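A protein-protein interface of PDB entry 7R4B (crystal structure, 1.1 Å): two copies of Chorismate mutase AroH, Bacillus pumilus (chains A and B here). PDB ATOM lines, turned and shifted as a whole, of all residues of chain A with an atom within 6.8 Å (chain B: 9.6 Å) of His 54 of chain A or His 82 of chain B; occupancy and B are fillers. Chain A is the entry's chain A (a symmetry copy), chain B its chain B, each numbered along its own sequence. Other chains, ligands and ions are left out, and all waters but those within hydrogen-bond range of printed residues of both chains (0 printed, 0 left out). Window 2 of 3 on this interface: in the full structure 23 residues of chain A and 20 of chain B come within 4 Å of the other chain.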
ATOM      1  N   ASP A  15      17.150 -24.046  -2.555  1.00  0.00           N
ATOM      2  CA  ASP A  15      17.892 -22.793  -2.666  1.00  0.00           C
ATOM      3  C   ASP A  15      18.546 -22.447  -1.332  1.00  0.00           C
ATOM      4  O   ASP A  15      18.089 -21.595  -0.567  1.00  0.00           O
ATOM      5  CB  ASP A  15      16.968 -21.678  -3.132  1.00  0.00           C
ATOM      6  CG  ASP A  15      17.680 -20.353  -3.251  1.00  0.00           C
ATOM      7  OD1 ASP A  15      18.915 -20.350  -3.446  1.00  0.00           O
ATOM      8  OD2 ASP A  15      17.009 -19.310  -3.160  1.00  0.00           O
ATOM      9  N   VAL A  20      23.787 -24.627  -3.428  1.00  0.00           N
ATOM     10  CA  VAL A  20      24.181 -23.900  -4.635  1.00  0.00           C
ATOM     11  C   VAL A  20      25.691 -23.986  -4.849  1.00  0.00           C
ATOM     12  O   VAL A  20      26.164 -24.314  -5.943  1.00  0.00           O
ATOM     13  CB  VAL A  20      23.688 -22.446  -4.566  1.00  0.00           C
ATOM     14  CG1 VAL A  20      24.283 -21.621  -5.703  1.00  0.00           C
ATOM     15  CG2 VAL A  20      22.169 -22.404  -4.626  1.00  0.00           C
ATOM     16  N   THR A  50      18.248 -20.006 -12.720  1.00  0.00           N
ATOM     17  CA  THR A  50      16.830 -19.717 -12.807  1.00  0.00           C
ATOM     18  C   THR A  50      16.441 -18.756 -11.681  1.00  0.00           C
ATOM     19  O   THR A  50      17.163 -18.585 -10.695  1.00  0.00           O
ATOM     20  CB  THR A  50      16.035 -21.014 -12.796  1.00  0.00           C
ATOM     21  OG1 THR A  50      16.544 -21.883 -11.774  1.00  0.00           O
ATOM     22  CG2 THR A  50      16.190 -21.733 -14.126  1.00  0.00           C
ATOM     23  N   GLN A  51      15.282 -18.118 -11.844  1.00  0.00           N
ATOM     24  CA  GLN A  51      14.851 -17.020 -10.976  1.00  0.00           C
ATOM     25  C   GLN A  51      14.250 -17.498  -9.664  1.00  0.00           C
ATOM     26  O   GLN A  51      13.630 -16.703  -8.936  1.00  0.00           O
ATOM     27  CB  GLN A  51      13.942 -16.071 -11.757  1.00  0.00           C
ATOM     28  CG  GLN A  51      14.652 -15.493 -12.974  1.00  0.00           C
ATOM     29  CD  GLN A  51      13.716 -14.752 -13.905  1.00  0.00           C
ATOM     30  OE1 GLN A  51      12.772 -14.108 -13.457  1.00  0.00           O
ATOM     31  NE2 GLN A  51      13.980 -14.831 -15.211  1.00  0.00           N
ATOM     32  N   ASP A  52      14.456 -18.773  -9.341  1.00  0.00           N
ATOM     33  CA  ASP A  52      14.125 -19.337  -8.043  1.00  0.00           C
ATOM     34  C   ASP A  52      15.365 -19.591  -7.184  1.00  0.00           C
ATOM     35  O   ASP A  52      15.275 -20.306  -6.172  1.00  0.00           O
ATOM     36  CB  ASP A  52      13.348 -20.641  -8.241  1.00  0.00           C
ATOM     37  CG  ASP A  52      14.039 -21.612  -9.177  1.00  0.00           C
ATOM     38  OD1 ASP A  52      15.223 -21.375  -9.502  1.00  0.00           O
ATOM     39  OD2 ASP A  52      13.395 -22.599  -9.589  1.00  0.00           O
ATOM     40  N   ILE A  53      16.514 -19.020  -7.553  1.00  0.00           N
ATOM     41  CA  ILE A  53      17.745 -19.148  -6.782  1.00  0.00           C
ATOM     42  C   ILE A  53      18.175 -17.765  -6.307  1.00  0.00           C
ATOM     43  O   ILE A  53      18.506 -16.892  -7.119  1.00  0.00           O
ATOM     44  CB  ILE A  53      18.851 -19.840  -7.593  1.00  0.00           C
ATOM     45  CG1 ILE A  53      18.463 -21.310  -7.785  1.00  0.00           C
ATOM     46  CG2 ILE A  53      20.178 -19.711  -6.871  1.00  0.00           C
ATOM     47  CD1 ILE A  53      19.238 -22.019  -8.852  1.00  0.00           C
ATOM     48  N   HIS A  54      18.203 -17.582  -4.991  1.00  0.00           N
ATOM     49  CA  HIS A  54      18.522 -16.291  -4.401  1.00  0.00           C
ATOM     50  C   HIS A  54      19.520 -16.366  -3.255  1.00  0.00           C
ATOM     51  O   HIS A  54      19.861 -15.320  -2.694  1.00  0.00           O
ATOM     52  CB  HIS A  54      17.251 -15.608  -3.869  1.00  0.00           C
ATOM     53  CG  HIS A  54      16.138 -15.560  -4.866  1.00  0.00           C
ATOM     54  ND1 HIS A  54      16.163 -14.709  -5.951  1.00  0.00           N
ATOM     55  CD2 HIS A  54      14.997 -16.282  -4.979  1.00  0.00           C
ATOM     56  CE1 HIS A  54      15.075 -14.890  -6.676  1.00  0.00           C
ATOM     57  NE2 HIS A  54      14.349 -15.838  -6.108  1.00  0.00           N
ATOM     58  N   SER A  55      19.981 -17.558  -2.877  1.00  0.00           N
ATOM     59  CA  SER A  55      20.739 -17.672  -1.633  1.00  0.00           C
ATOM     60  C   SER A  55      22.172 -17.173  -1.745  1.00  0.00           C
ATOM     61  O   SER A  55      22.712 -16.651  -0.767  1.00  0.00           O
ATOM     62  CB  SER A  55      20.715 -19.111  -1.118  1.00  0.00           C
ATOM     63  OG  SER A  55      21.320 -19.994  -2.034  1.00  0.00           O
ATOM     64  N   VAL A  56      22.799 -17.301  -2.917  1.00  0.00           N
ATOM     65  CA  VAL A  56      24.213 -16.977  -3.094  1.00  0.00           C
ATOM     66  C   VAL A  56      24.478 -16.888  -4.590  1.00  0.00           C
ATOM     67  O   VAL A  56      23.805 -17.557  -5.381  1.00  0.00           O
ATOM     68  CB  VAL A  56      25.100 -18.052  -2.437  1.00  0.00           C
ATOM     69  CG1 VAL A  56      24.980 -19.414  -3.150  1.00  0.00           C
ATOM     70  CG2 VAL A  56      26.551 -17.587  -2.376  1.00  0.00           C
ATOM     71  N   PHE A  57      25.439 -16.056  -4.996  1.00  0.00           N
ATOM     72  CA  PHE A  57      25.883 -16.083  -6.386  1.00  0.00           C
ATOM     73  C   PHE A  57      26.619 -17.392  -6.641  1.00  0.00           C
ATOM     74  O   PHE A  57      27.561 -17.701  -5.905  1.00  0.00           O
ATOM     75  CB  PHE A  57      26.849 -14.935  -6.694  1.00  0.00           C
ATOM     76  CG  PHE A  57      26.182 -13.627  -6.914  1.00  0.00           C
ATOM     77  CD1 PHE A  57      25.513 -13.375  -8.105  1.00  0.00           C
ATOM     78  CD2 PHE A  57      26.227 -12.636  -5.946  1.00  0.00           C
ATOM     79  CE1 PHE A  57      24.874 -12.175  -8.310  1.00  0.00           C
ATOM     80  CE2 PHE A  57      25.596 -11.414  -6.160  1.00  0.00           C
ATOM     81  CZ  PHE A  57      24.914 -11.198  -7.337  1.00  0.00           C
ATOM     82  N   GLN A  77      20.533 -13.894 -14.939  1.00  0.00           N
ATOM     83  CA  GLN A  77      19.288 -14.632 -14.784  1.00  0.00           C
ATOM     84  C   GLN A  77      18.965 -15.399 -16.062  1.00  0.00           C
ATOM     85  O   GLN A  77      19.086 -14.874 -17.169  1.00  0.00           O
ATOM     86  CB  GLN A  77      18.150 -13.657 -14.503  1.00  0.00           C
ATOM     87  CG  GLN A  77      18.150 -13.031 -13.112  1.00  0.00           C
ATOM     88  CD  GLN A  77      16.915 -12.175 -12.850  1.00  0.00           C
ATOM     89  OE1 GLN A  77      15.911 -12.288 -13.545  1.00  0.00           O
ATOM     90  NE2 GLN A  77      16.999 -11.289 -11.867  1.00  0.00           N
ATOM     91  N   GLN B  51      17.854  -6.013 -10.943  1.00  0.00           N
ATOM     92  CA  GLN B  51      16.489  -5.875 -11.421  1.00  0.00           C
ATOM     93  C   GLN B  51      15.776  -4.648 -10.858  1.00  0.00           C
ATOM     94  O   GLN B  51      14.584  -4.464 -11.132  1.00  0.00           O
ATOM     95  CB  GLN B  51      15.704  -7.156 -11.163  1.00  0.00           C
ATOM     96  CG  GLN B  51      15.461  -7.498  -9.715  1.00  0.00           C
ATOM     97  CD  GLN B  51      14.809  -8.885  -9.545  1.00  0.00           C
ATOM     98  OE1 GLN B  51      15.083  -9.826 -10.305  1.00  0.00           O
ATOM     99  NE2 GLN B  51      13.953  -9.013  -8.538  1.00  0.00           N
ATOM    100  N   GLN B  77      19.960  -9.253 -17.252  1.00  0.00           N
ATOM    101  CA  GLN B  77      19.570  -9.026 -15.873  1.00  0.00           C
ATOM    102  C   GLN B  77      20.387  -9.901 -14.929  1.00  0.00           C
ATOM    103  O   GLN B  77      20.488 -11.113 -15.117  1.00  0.00           O
ATOM    104  CB  GLN B  77      18.084  -9.306 -15.698  1.00  0.00           C
ATOM    105  CG  GLN B  77      17.519  -8.774 -14.379  1.00  0.00           C
ATOM    106  CD  GLN B  77      16.079  -8.392 -14.470  1.00  0.00           C
ATOM    107  OE1 GLN B  77      15.742  -7.253 -14.782  1.00  0.00           O
ATOM    108  NE2 GLN B  77      15.211  -9.366 -14.246  1.00  0.00           N
ATOM    109  N   GLU B  78      20.970  -9.271 -13.922  1.00  0.00           N
ATOM    110  CA  GLU B  78      21.715  -9.964 -12.888  1.00  0.00           C
ATOM    111  C   GLU B  78      20.768 -10.681 -11.923  1.00  0.00           C
ATOM    112  O   GLU B  78      19.610 -10.285 -11.737  1.00  0.00           O
ATOM    113  CB  GLU B  78      22.565  -8.933 -12.133  1.00  0.00           C
ATOM    114  CG  GLU B  78      23.348  -9.452 -10.933  1.00  0.00           C
ATOM    115  CD  GLU B  78      24.399 -10.510 -11.289  1.00  0.00           C
ATOM    116  OE1 GLU B  78      24.058 -11.653 -11.672  1.00  0.00           O
ATOM    117  OE2 GLU B  78      25.587 -10.188 -11.114  1.00  0.00           O
ATOM    118  N   LEU B  79      21.273 -11.757 -11.315  1.00  0.00           N
ATOM    119  CA  LEU B  79      20.528 -12.468 -10.286  1.00  0.00           C
ATOM    120  C   LEU B  79      20.150 -11.543  -9.140  1.00  0.00           C
ATOM    121  O   LEU B  79      20.857 -10.584  -8.813  1.00  0.00           O
ATOM    122  CB  LEU B  79      21.374 -13.605  -9.731  1.00  0.00           C
ATOM    123  CG  LEU B  79      21.903 -14.616 -10.732  1.00  0.00           C
ATOM    124  CD1 LEU B  79      22.757 -15.699 -10.068  1.00  0.00           C
ATOM    125  CD2 LEU B  79      20.778 -15.275 -11.516  1.00  0.00           C
ATOM    126  N   ASP B  80      19.042 -11.883  -8.493  1.00  0.00           N
ATOM    127  CA  ASP B  80      18.593 -11.181  -7.295  1.00  0.00           C
ATOM    128  C   ASP B  80      18.995 -12.061  -6.112  1.00  0.00           C
ATOM    129  O   ASP B  80      18.280 -12.974  -5.713  1.00  0.00           O
ATOM    130  CB  ASP B  80      17.093 -10.976  -7.356  1.00  0.00           C
ATOM    131  CG  ASP B  80      16.544 -10.365  -6.094  1.00  0.00           C
ATOM    132  OD1 ASP B  80      17.287  -9.607  -5.434  1.00  0.00           O
ATOM    133  OD2 ASP B  80      15.387 -10.666  -5.755  1.00  0.00           O
ATOM    134  N   ILE B  81      20.158 -11.772  -5.537  1.00  0.00           N
ATOM    135  CA  ILE B  81      20.727 -12.542  -4.434  1.00  0.00           C
ATOM    136  C   ILE B  81      20.459 -11.788  -3.142  1.00  0.00           C
ATOM    137  O   ILE B  81      20.699 -10.580  -3.041  1.00  0.00           O
ATOM    138  CB  ILE B  81      22.230 -12.773  -4.642  1.00  0.00           C
ATOM    139  CG1 ILE B  81      22.486 -13.551  -5.942  1.00  0.00           C
ATOM    140  CG2 ILE B  81      22.837 -13.490  -3.442  1.00  0.00           C
ATOM    141  CD1 ILE B  81      21.724 -14.861  -6.069  1.00  0.00           C
ATOM    142  N   HIS B  82      19.937 -12.487  -2.149  1.00  0.00           N
ATOM    143  CA  HIS B  82      19.615 -11.809  -0.903  1.00  0.00           C
ATOM    144  C   HIS B  82      20.923 -11.321  -0.281  1.00  0.00           C
ATOM    145  O   HIS B  82      21.882 -12.079  -0.159  1.00  0.00           O
ATOM    146  CB  HIS B  82      18.849 -12.750   0.024  1.00  0.00           C
ATOM    147  CG  HIS B  82      17.559 -13.274  -0.559  1.00  0.00           C
ATOM    148  ND1 HIS B  82      16.703 -12.506  -1.328  1.00  0.00           N
ATOM    149  CD2 HIS B  82      16.946 -14.475  -0.409  1.00  0.00           C
ATOM    150  CE1 HIS B  82      15.645 -13.229  -1.659  1.00  0.00           C
ATOM    151  NE2 HIS B  82      15.774 -14.429  -1.123  1.00  0.00           N
ATOM    152  N   GLY B  83      20.991 -10.031   0.041  1.00  0.00           N
ATOM    153  CA  GLY B  83      22.227  -9.418   0.490  1.00  0.00           C
ATOM    154  C   GLY B  83      23.129  -8.907  -0.613  1.00  0.00           C
ATOM    155  O   GLY B  83      24.149  -8.261  -0.320  1.00  0.00           O
ATOM    156  N   GLY B  84      22.786  -9.161  -1.865  1.00  0.00           N
ATOM    157  CA  GLY B  84      23.569  -8.647  -2.962  1.00  0.00           C
ATOM    158  C   GLY B  84      23.457  -7.142  -3.093  1.00  0.00           C
ATOM    159  O   GLY B  84      22.496  -6.506  -2.663  1.00  0.00           O
ATOM    160  N   LEU B  85      24.473  -6.564  -3.711  1.00  0.00           N
ATOM    161  CA  LEU B  85      24.537  -5.122  -3.885  1.00  0.00           C
ATOM    162  C   LEU B  85      23.382  -4.650  -4.757  1.00  0.00           C
ATOM    163  O   LEU B  85      23.119  -5.200  -5.825  1.00  0.00           O
ATOM    164  CB  LEU B  85      25.875  -4.783  -4.537  1.00  0.00           C
ATOM    165  CG  LEU B  85      26.501  -3.418  -4.306  1.00  0.00           C
ATOM    166  CD1 LEU B  85      26.618  -3.032  -2.846  1.00  0.00           C
ATOM    167  CD2 LEU B  85      27.865  -3.440  -4.982  1.00  0.00           C
ATOM    168  N   LYS B  86      22.692  -3.625  -4.296  1.00  0.00           N
ATOM    169  CA  LYS B  86      21.597  -3.055  -5.060  1.00  0.00           C
ATOM    170  C   LYS B  86      22.116  -2.042  -6.075  1.00  0.00           C
ATOM    171  O   LYS B  86      23.238  -1.525  -5.970  1.00  0.00           O
ATOM    172  CB  LYS B  86      20.587  -2.382  -4.120  1.00  0.00           C
ATOM    173  CG  LYS B  86      20.143  -3.270  -2.972  1.00  0.00           C
ATOM    174  CD  LYS B  86      19.356  -4.468  -3.456  1.00  0.00           C
ATOM    175  CE  LYS B  86      18.201  -4.822  -2.484  1.00  0.00           C
ATOM    176  NZ  LYS B  86      17.778  -6.240  -2.608  1.00  0.00           N
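NE2 of Gln 77 of chain A is in hydrogen-bond range of O of Glu 78 of chain B, 2.8 Å away. The side-chain amide oxygen of Gln 51 of chain B lies within hydrogen-bond range of the side-chain amide nitrogen of Gln 77 of chain A (2.9 Å). The backbone carbonyl oxygen of Gln 77 of chain B sits at hydrogen-bond distance from the backbone NH of Gln 77 of chain A (2.8 Å). A ring nitrogen (ND1) of His 54 of chain A is in hydrogen-bond range of the backbone carbonyl oxygen (O) of Asp 80 of chain B, at 2.7 Å. The backbone NH (N) of His 82 of chain B is in hydrogen-bond range of the backbone carbonyl oxygen (O) of His 54 of chain A, at 2.9 Å.
Among the printed residues, pairs that only touch across the chains: His 54 of chain A with Ile 81 of chain B (3.4 Å), Phe 57 of chain A with Glu 78 of chain B (3.4 Å), Val 56 of chain A with Ile 81 of chain B (3.5 Å), Phe 57 of chain A with Ile 81 of chain B (3.6 Å), Gln 77 of chain A with Leu 79 of chain B (3.6 Å), Ile 53 of chain A with Ile 81 of chain B (3.9 Å) and Gln 77 of chain A with Asp 80 of chain B (3.99 Å).
Of the printed residues of chain B, His 54 of chain A touches Asp 80 (2.7 Å), Ile 81 (3.4 Å) and His 82 (2.9 Å). Of chain A, only His 54 comes within 4 Å of His 82 of chain B. Of the printed residues of chain A, Leu 79 of chain B touches Gln 77 (3.6 Å). Of the printed residues of chain B, Gln 77 of chain A touches Gln 51, Gln 77, Glu 78, Leu 79 and Asp 80. Of the printed residues of chain A, Ile 81 of chain B touches Ile 53 (3.9 Å), His 54 (3.4 Å), Val 56 (3.5 Å) and Phe 57 (3.6 Å). Asp 52 of chain A touches none of the printed residues of chain B. The nearest residue of chain A that does not touch His 82 of chain B is Ser 55 of chain A (4.7 Å). The nearest printed residue of chain A that does not touch Ile 81 of chain B is Ser 55 of chain A (4.1 Å).
Gln 77 of chain A touches Gln 51 of chain B, but with the chains exchanged Gln 51 of chain A does not touch Gln 77 of chain B (5.4 Å). Gln 77 of chain B touches its own counterpart, Gln 77 of chain A.
The side-chain carboxylate of Asp 15 of chain A is in hydrogen-bond range of the backbone NH of His 54 of chain A (2.8 Å). A ring nitrogen (NE2) of His 54 of chain A is in hydrogen-bond range of the backbone carbonyl oxygen of Gln 51 of chain A (3.0 Å).
Printed residues of chain A that touch a printed residue of chain B: Ile 53, His 54, Val 56, Phe 57 and Gln 77. Of the 11 printed residues of chain B, 7 touch a printed residue of chain A. Hydrophobic or aromatic side chains of chain B that line the printed part of chain A: Leu 79, Ile 81 and His 82. Among the printed residues, 12 pairs touch across the chains. Among the printed residues, no Asp or Glu carboxylate lies within 4 Å of a Lys or Arg side-chain nitrogen of the other chain.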
